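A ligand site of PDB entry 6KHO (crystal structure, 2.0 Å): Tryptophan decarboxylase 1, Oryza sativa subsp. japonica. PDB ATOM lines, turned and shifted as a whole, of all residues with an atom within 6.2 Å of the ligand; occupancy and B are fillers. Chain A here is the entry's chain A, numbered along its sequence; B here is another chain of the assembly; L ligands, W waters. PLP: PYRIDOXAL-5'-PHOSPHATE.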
ATOM      1  N   PHE A 104      14.893 -14.961  -1.779  1.00  0.00           N
ATOM      2  CA  PHE A 104      15.566 -14.247  -0.697  1.00  0.00           C
ATOM      3  C   PHE A 104      14.975 -12.845  -0.610  1.00  0.00           C
ATOM      4  O   PHE A 104      14.576 -12.291  -1.629  1.00  0.00           O
ATOM      5  CB  PHE A 104      17.083 -14.164  -0.912  1.00  0.00           C
ATOM      6  CG  PHE A 104      17.778 -15.501  -0.910  1.00  0.00           C
ATOM      7  CD1 PHE A 104      17.779 -16.301   0.221  1.00  0.00           C
ATOM      8  CD2 PHE A 104      18.417 -15.951  -2.057  1.00  0.00           C
ATOM      9  CE1 PHE A 104      18.429 -17.532   0.211  1.00  0.00           C
ATOM     10  CE2 PHE A 104      19.059 -17.188  -2.070  1.00  0.00           C
ATOM     11  CZ  PHE A 104      19.054 -17.980  -0.938  1.00  0.00           C
ATOM     12  N   GLY A 173      24.479  -4.540 -12.478  1.00  0.00           N
ATOM     13  CA  GLY A 173      23.088  -4.738 -12.119  1.00  0.00           C
ATOM     14  C   GLY A 173      22.805  -6.099 -11.522  1.00  0.00           C
ATOM     15  O   GLY A 173      22.012  -6.222 -10.585  1.00  0.00           O
ATOM     16  N   THR A 174      23.457  -7.150 -12.028  1.00  0.00           N
ATOM     17  CA  THR A 174      23.039  -8.524 -11.720  1.00  0.00           C
ATOM     18  C   THR A 174      24.242  -9.443 -11.580  1.00  0.00           C
ATOM     19  O   THR A 174      25.319  -9.200 -12.134  1.00  0.00           O
ATOM     20  CB  THR A 174      22.129  -9.121 -12.826  1.00  0.00           C
ATOM     21  OG1 THR A 174      22.834  -9.121 -14.080  1.00  0.00           O
ATOM     22  CG2 THR A 174      20.817  -8.332 -12.967  1.00  0.00           C
ATOM     23  N   THR A 175      24.016 -10.552 -10.878  1.00  0.00           N
ATOM     24  CA  THR A 175      25.016 -11.618 -10.849  1.00  0.00           C
ATOM     25  C   THR A 175      25.236 -12.194 -12.242  1.00  0.00           C
ATOM     26  O   THR A 175      26.365 -12.551 -12.605  1.00  0.00           O
ATOM     27  CB  THR A 175      24.590 -12.701  -9.856  1.00  0.00           C
ATOM     28  OG1 THR A 175      24.644 -12.152  -8.527  1.00  0.00           O
ATOM     29  CG2 THR A 175      25.535 -13.909  -9.907  1.00  0.00           C
ATOM     30  N   SER A 176      24.181 -12.249 -13.068  1.00  0.00           N
ATOM     31  CA  SER A 176      24.347 -12.783 -14.418  1.00  0.00           C
ATOM     32  C   SER A 176      25.395 -12.005 -15.216  1.00  0.00           C
ATOM     33  O   SER A 176      26.226 -12.613 -15.900  1.00  0.00           O
ATOM     34  CB  SER A 176      23.012 -12.791 -15.165  1.00  0.00           C
ATOM     35  OG  SER A 176      22.052 -13.567 -14.459  1.00  0.00           O
ATOM     36  N   GLU A 177      25.351 -10.659 -15.155  1.00  0.00           N
ATOM     37  CA  GLU A 177      26.362  -9.882 -15.865  1.00  0.00           C
ATOM     38  C   GLU A 177      27.755 -10.120 -15.290  1.00  0.00           C
ATOM     39  O   GLU A 177      28.744 -10.143 -16.028  1.00  0.00           O
ATOM     40  CB  GLU A 177      26.031  -8.383 -15.826  1.00  0.00           C
ATOM     41  CG  GLU A 177      26.947  -7.579 -16.800  1.00  0.00           C
ATOM     42  CD  GLU A 177      26.579  -6.112 -16.908  1.00  0.00           C
ATOM     43  OE1 GLU A 177      25.580  -5.698 -16.258  1.00  0.00           O
ATOM     44  OE2 GLU A 177      27.275  -5.376 -17.646  1.00  0.00           O
ATOM     45  N   MET A 179      28.781 -12.903 -13.951  1.00  0.00           N
ATOM     46  CA  MET A 179      29.181 -14.184 -14.500  1.00  0.00           C
ATOM     47  C   MET A 179      29.573 -14.052 -15.950  1.00  0.00           C
ATOM     48  O   MET A 179      30.576 -14.629 -16.388  1.00  0.00           O
ATOM     49  CB  MET A 179      28.040 -15.193 -14.355  1.00  0.00           C
ATOM     50  CG  MET A 179      27.873 -15.705 -12.942  1.00  0.00           C
ATOM     51  SD  MET A 179      26.296 -16.553 -12.753  1.00  0.00           S
ATOM     52  CE  MET A 179      26.476 -17.170 -11.072  1.00  0.00           C
ATOM     53  N   HIS A 214      22.986 -21.482  -9.426  1.00  0.00           N
ATOM     54  CA  HIS A 214      21.828 -20.798  -9.985  1.00  0.00           C
ATOM     55  C   HIS A 214      21.751 -20.991 -11.494  1.00  0.00           C
ATOM     56  O   HIS A 214      22.772 -20.971 -12.188  1.00  0.00           O
ATOM     57  CB  HIS A 214      21.886 -19.316  -9.643  1.00  0.00           C
ATOM     58  CG  HIS A 214      20.558 -18.622  -9.715  1.00  0.00           C
ATOM     59  ND1 HIS A 214      19.998 -18.202 -10.898  1.00  0.00           N
ATOM     60  CD2 HIS A 214      19.676 -18.289  -8.748  1.00  0.00           C
ATOM     61  CE1 HIS A 214      18.839 -17.626 -10.655  1.00  0.00           C
ATOM     62  NE2 HIS A 214      18.613 -17.666  -9.360  1.00  0.00           N
ATOM     63  N   THR A 216      21.038 -19.150 -13.781  1.00  0.00           N
ATOM     64  CA  THR A 216      21.559 -18.047 -14.582  1.00  0.00           C
ATOM     65  C   THR A 216      23.022 -18.230 -14.967  1.00  0.00           C
ATOM     66  O   THR A 216      23.464 -17.634 -15.964  1.00  0.00           O
ATOM     67  CB  THR A 216      21.365 -16.729 -13.833  1.00  0.00           C
ATOM     68  OG1 THR A 216      21.382 -15.653 -14.776  1.00  0.00           O
ATOM     69  CG2 THR A 216      22.442 -16.516 -12.763  1.00  0.00           C
ATOM     70  N   THR A 269      29.731 -21.669  -5.453  1.00  0.00           N
ATOM     71  CA  THR A 269      28.680 -20.864  -4.834  1.00  0.00           C
ATOM     72  C   THR A 269      28.765 -20.955  -3.316  1.00  0.00           C
ATOM     73  O   THR A 269      28.826 -22.059  -2.752  1.00  0.00           O
ATOM     74  CB  THR A 269      27.281 -21.308  -5.296  1.00  0.00           C
ATOM     75  OG1 THR A 269      27.190 -21.161  -6.710  1.00  0.00           O
ATOM     76  CG2 THR A 269      26.182 -20.432  -4.637  1.00  0.00           C
ATOM     77  N   VAL A 270      28.760 -19.797  -2.662  1.00  0.00           N
ATOM     78  CA  VAL A 270      28.637 -19.706  -1.211  1.00  0.00           C
ATOM     79  C   VAL A 270      27.219 -19.228  -0.920  1.00  0.00           C
ATOM     80  O   VAL A 270      26.914 -18.035  -1.060  1.00  0.00           O
ATOM     81  CB  VAL A 270      29.691 -18.777  -0.591  1.00  0.00           C
ATOM     82  CG1 VAL A 270      29.468 -18.655   0.917  1.00  0.00           C
ATOM     83  CG2 VAL A 270      31.085 -19.309  -0.887  1.00  0.00           C
ATOM     84  N   GLY A 271      26.345 -20.152  -0.505  1.00  0.00           N
ATOM     85  CA  GLY A 271      24.955 -19.811  -0.240  1.00  0.00           C
ATOM     86  C   GLY A 271      24.046 -20.072  -1.425  1.00  0.00           C
ATOM     87  O   GLY A 271      23.497 -19.136  -2.016  1.00  0.00           O
ATOM     88  N   THR A 272      23.863 -21.333  -1.784  1.00  0.00           N
ATOM     89  CA  THR A 272      23.075 -21.641  -2.975  1.00  0.00           C
ATOM     90  C   THR A 272      21.619 -21.227  -2.785  1.00  0.00           C
ATOM     91  O   THR A 272      21.122 -21.130  -1.669  1.00  0.00           O
ATOM     92  CB  THR A 272      23.123 -23.135  -3.307  1.00  0.00           C
ATOM     93  OG1 THR A 272      22.549 -23.865  -2.221  1.00  0.00           O
ATOM     94  CG2 THR A 272      24.561 -23.615  -3.576  1.00  0.00           C
ATOM     95  N   THR A 273      20.936 -21.030  -3.911  1.00  0.00           N
ATOM     96  CA  THR A 273      19.576 -20.511  -3.882  1.00  0.00           C
ATOM     97  C   THR A 273      18.606 -21.509  -3.257  1.00  0.00           C
ATOM     98  O   THR A 273      17.715 -21.119  -2.486  1.00  0.00           O
ATOM     99  CB  THR A 273      19.127 -20.141  -5.290  1.00  0.00           C
ATOM    100  OG1 THR A 273      19.996 -19.143  -5.823  1.00  0.00           O
ATOM    101  CG2 THR A 273      17.715 -19.608  -5.284  1.00  0.00           C
ATOM    102  N   ASP A 298      30.337 -17.200  -6.588  1.00  0.00           N
ATOM    103  CA  ASP A 298      29.020 -16.551  -6.545  1.00  0.00           C
ATOM    104  C   ASP A 298      28.534 -16.565  -5.101  1.00  0.00           C
ATOM    105  O   ASP A 298      28.173 -17.626  -4.570  1.00  0.00           O
ATOM    106  CB  ASP A 298      28.024 -17.291  -7.436  1.00  0.00           C
ATOM    107  CG  ASP A 298      26.577 -16.734  -7.326  1.00  0.00           C
ATOM    108  OD1 ASP A 298      26.365 -15.644  -6.745  1.00  0.00           O
ATOM    109  OD2 ASP A 298      25.657 -17.392  -7.848  1.00  0.00           O
ATOM    110  N   ALA A 299      28.547 -15.394  -4.453  1.00  0.00           N
ATOM    111  CA  ALA A 299      28.059 -15.248  -3.087  1.00  0.00           C
ATOM    112  C   ALA A 299      26.954 -14.208  -3.032  1.00  0.00           C
ATOM    113  O   ALA A 299      26.897 -13.385  -2.119  1.00  0.00           O
ATOM    114  CB  ALA A 299      29.180 -14.876  -2.129  1.00  0.00           C
ATOM    115  N   ALA A 300      26.047 -14.271  -4.006  1.00  0.00           N
ATOM    116  CA  ALA A 300      25.056 -13.209  -4.232  1.00  0.00           C
ATOM    117  C   ALA A 300      24.289 -12.856  -2.967  1.00  0.00           C
ATOM    118  O   ALA A 300      24.095 -11.679  -2.664  1.00  0.00           O
ATOM    119  CB  ALA A 300      24.089 -13.636  -5.337  1.00  0.00           C
ATOM    120  N   TYR A 301      23.847 -13.867  -2.228  1.00  0.00           N
ATOM    121  CA  TYR A 301      23.075 -13.688  -1.004  1.00  0.00           C
ATOM    122  C   TYR A 301      23.967 -13.708   0.229  1.00  0.00           C
ATOM    123  O   TYR A 301      24.031 -12.725   0.986  1.00  0.00           O
ATOM    124  CB  TYR A 301      22.015 -14.794  -0.901  1.00  0.00           C
ATOM    125  CG  TYR A 301      21.400 -14.955   0.473  1.00  0.00           C
ATOM    126  CD1 TYR A 301      20.484 -14.023   0.971  1.00  0.00           C
ATOM    127  CD2 TYR A 301      21.716 -16.063   1.254  1.00  0.00           C
ATOM    128  CE1 TYR A 301      19.907 -14.190   2.225  1.00  0.00           C
ATOM    129  CE2 TYR A 301      21.155 -16.231   2.498  1.00  0.00           C
ATOM    130  CZ  TYR A 301      20.245 -15.304   2.986  1.00  0.00           C
ATOM    131  OH  TYR A 301      19.696 -15.488   4.229  1.00  0.00           O
ATOM    132  N   SER A 327      25.640  -9.504  -3.890  1.00  0.00           N
ATOM    133  CA  SER A 327      24.607  -8.513  -4.188  1.00  0.00           C
ATOM    134  C   SER A 327      24.148  -7.834  -2.915  1.00  0.00           C
ATOM    135  O   SER A 327      23.404  -8.439  -2.112  1.00  0.00           O
ATOM    136  CB  SER A 327      23.423  -9.163  -4.906  1.00  0.00           C
ATOM    137  OG  SER A 327      23.815  -9.576  -6.200  1.00  0.00           O
ATOM    138  N   HIS A 329      21.918  -5.842  -3.002  1.00  0.00           N
ATOM    139  CA  HIS A 329      20.460  -5.762  -3.136  1.00  0.00           C
ATOM    140  C   HIS A 329      19.752  -7.029  -2.685  1.00  0.00           C
ATOM    141  O   HIS A 329      18.518  -7.079  -2.757  1.00  0.00           O
ATOM    142  CB  HIS A 329      20.056  -5.355  -4.572  1.00  0.00           C
ATOM    143  CG  HIS A 329      20.216  -6.435  -5.611  1.00  0.00           C
ATOM    144  ND1 HIS A 329      20.808  -6.199  -6.827  1.00  0.00           N
ATOM    145  CD2 HIS A 329      19.790  -7.730  -5.647  1.00  0.00           C
ATOM    146  CE1 HIS A 329      20.774  -7.287  -7.562  1.00  0.00           C
ATOM    147  NE2 HIS A 329      20.160  -8.230  -6.871  1.00  0.00           N
ATOM    148  N   LYS A 330      20.480  -8.031  -2.210  1.00  0.00           N
ATOM    149  CA  LYS A 330      19.838  -9.123  -1.494  1.00  0.00           C
ATOM    150  C   LYS A 330      19.780  -8.776  -0.019  1.00  0.00           C
ATOM    151  O   LYS A 330      18.761  -8.306   0.476  1.00  0.00           O
ATOM    152  CB  LYS A 330      20.584 -10.444  -1.709  1.00  0.00           C
ATOM    153  CG  LYS A 330      20.546 -10.905  -3.140  1.00  0.00           C
ATOM    154  CD  LYS A 330      19.550 -11.999  -3.336  1.00  0.00           C
ATOM    155  CE  LYS A 330      20.060 -12.970  -4.380  1.00  0.00           C
ATOM    156  NZ  LYS A 330      19.008 -13.318  -5.334  1.00  0.00           N
ATOM    157  N   THR A 339      24.886  -5.198  -7.649  1.00  0.00           N
ATOM    158  CA  THR A 339      25.733  -6.380  -7.500  1.00  0.00           C
ATOM    159  C   THR A 339      27.183  -5.934  -7.621  1.00  0.00           C
ATOM    160  O   THR A 339      27.515  -5.191  -8.547  1.00  0.00           O
ATOM    161  CB  THR A 339      25.431  -7.433  -8.571  1.00  0.00           C
ATOM    162  OG1 THR A 339      24.064  -7.829  -8.470  1.00  0.00           O
ATOM    163  CG2 THR A 339      26.326  -8.686  -8.380  1.00  0.00           C
ATOM    164  N   VAL B 378      20.111 -10.277 -20.053  1.00  0.00           N
ATOM    165  CA  VAL B 378      21.254 -10.998 -19.484  1.00  0.00           C
ATOM    166  C   VAL B 378      20.878 -11.617 -18.132  1.00  0.00           C
ATOM    167  O   VAL B 378      21.017 -12.828 -17.933  1.00  0.00           O
ATOM    168  CB  VAL B 378      22.494 -10.085 -19.391  1.00  0.00           C
ATOM    169  CG1 VAL B 378      23.042  -9.810 -20.768  1.00  0.00           C
ATOM    170  CG2 VAL B 378      22.160  -8.775 -18.703  1.00  0.00           C
ATOM    171  N   GLY B 379      20.351 -10.805 -17.209  1.00  0.00           N
ATOM    172  CA  GLY B 379      20.033 -11.267 -15.876  1.00  0.00           C
ATOM    173  C   GLY B 379      18.601 -11.766 -15.734  1.00  0.00           C
ATOM    174  O   GLY B 379      17.832 -11.816 -16.699  1.00  0.00           O
ATOM    175  N   VAL B 380      18.252 -12.172 -14.517  1.00  0.00           N
ATOM    176  CA  VAL B 380      16.896 -12.602 -14.195  1.00  0.00           C
ATOM    177  C   VAL B 380      16.190 -11.609 -13.264  1.00  0.00           C
ATOM    178  O   VAL B 380      15.113 -11.126 -13.569  1.00  0.00           O
ATOM    179  CB  VAL B 380      16.869 -14.045 -13.636  1.00  0.00           C
ATOM    180  CG1 VAL B 380      17.722 -14.970 -14.544  1.00  0.00           C
ATOM    181  CG2 VAL B 380      17.304 -14.134 -12.166  1.00  0.00           C
ATOM    182  N   GLY B 381      16.837 -11.243 -12.160  1.00  0.00           N
ATOM    183  CA  GLY B 381      16.217 -10.367 -11.204  1.00  0.00           C
ATOM    184  C   GLY B 381      16.701  -8.932 -11.232  1.00  0.00           C
ATOM    185  O   GLY B 381      17.807  -8.633 -10.747  1.00  0.00           O
ATOM    186  N   ARG B 382      15.873  -8.025 -11.740  1.00  0.00           N
ATOM    187  CA  ARG B 382      16.222  -6.609 -11.821  1.00  0.00           C
ATOM    188  C   ARG B 382      14.986  -5.767 -11.476  1.00  0.00           C
ATOM    189  O   ARG B 382      13.909  -6.298 -11.183  1.00  0.00           O
ATOM    190  CB  ARG B 382      16.770  -6.257 -13.212  1.00  0.00           C
ATOM    191  CG  ARG B 382      15.922  -6.804 -14.350  1.00  0.00           C
ATOM    192  CD  ARG B 382      14.996  -5.749 -14.920  1.00  0.00           C
ATOM    193  NE  ARG B 382      14.329  -6.201 -16.139  1.00  0.00           N
ATOM    194  CZ  ARG B 382      13.230  -5.656 -16.649  1.00  0.00           C
ATOM    195  NH1 ARG B 382      12.646  -4.618 -16.044  1.00  0.00           N
ATOM    196  NH2 ARG B 382      12.713  -6.150 -17.765  1.00  0.00           N
HETATM  197  N1  PLP L   1      23.053 -16.506  -7.602  1.00  0.00           N
HETATM  198  C2  PLP L   1      22.628 -16.644  -6.292  1.00  0.00           C
HETATM  199  C2A PLP L   1      23.347 -17.542  -5.331  1.00  0.00           C
HETATM  200  C3  PLP L   1      21.525 -15.942  -5.849  1.00  0.00           C
HETATM  201  O3  PLP L   1      21.108 -16.084  -4.559  1.00  0.00           O
HETATM  202  C4  PLP L   1      20.847 -15.089  -6.712  1.00  0.00           C
HETATM  203  C4A PLP L   1      19.907 -14.058  -6.153  1.00  0.00           C
HETATM  204  C5  PLP L   1      21.272 -14.951  -8.022  1.00  0.00           C
HETATM  205  C6  PLP L   1      22.374 -15.667  -8.469  1.00  0.00           C
HETATM  206  C5A PLP L   1      20.481 -14.026  -8.924  1.00  0.00           C
HETATM  207  O4P PLP L   1      21.136 -13.720 -10.136  1.00  0.00           O
HETATM  208  P   PLP L   1      20.797 -12.351 -10.944  1.00  0.00           P
HETATM  209  O1P PLP L   1      19.305 -12.189 -11.115  1.00  0.00           O
HETATM  210  O2P PLP L   1      21.493 -12.446 -12.283  1.00  0.00           O
HETATM  211  O3P PLP L   1      21.286 -11.128 -10.203  1.00  0.00           O
HETATM  212  O   HOH W   1      22.209 -11.151  -7.656  1.00  0.00           O
HETATM  213  O   HOH W   2      19.297 -10.005  -8.908  1.00  0.00           O
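The side-chain hydroxyl of Thr 273 lies within hydrogen-bond range of an oxygen (O3) of the ligand (3.5 Å).
An oxygen (O2P) of the ligand lies within hydrogen-bond range of the backbone NH of Ser 176, at 2.8 Å.
The side-chain amino group of Lys 330 is covalently linked to a carbon (C4A) of the ligand (1.4 Å).
OG of Ser 176 lies within hydrogen-bond range of O2P of the ligand (2.5 Å).
The backbone NH (N) of Gly 381 of chain B sits at hydrogen-bond distance from an oxygen (O1P) of the ligand (2.8 Å).
O3P of the ligand is in hydrogen-bond range of N of Thr 175.
The side-chain carboxylate (OD2) of Asp 298 is in hydrogen-bond range of a nitrogen (N1) of the ligand.
The backbone carbonyl oxygen (O) of Asp 298 lies within hydrogen-bond range of the backbone NH (N) of Val 270, 2.9 Å away.
The side-chain hydroxyl (OG1) of Thr 174 sits at hydrogen-bond distance from the backbone NH (N) of Glu 177, at 3.1 Å.
OD1 of Asp 298 is in hydrogen-bond range of N of Ala 300, 3.1 Å away.
N of Ser 327 lies within hydrogen-bond range of O of Ala 300 (2.9 Å).
A ring nitrogen (ND1) of His 214 sits close to the backbone NH (N) of Thr 216, 3.2 Å away.
Merely in contact with the ligand: Phe 104, Thr 174, His 214, Gly 271, Ala 300, Tyr 301 and Val 380 of chain B.
Water W2 lies within hydrogen-bond range of O3P of the ligand (2.6 Å), O of Gly 381 of chain B (2.7 Å) and NE2 of His 329 (2.8 Å).
Water W1 lies within hydrogen-bond range of the side-chain hydroxyl (OG) of Ser 327, an oxygen (O3P) of the ligand and the side-chain hydroxyl (OG1) of Thr 175.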
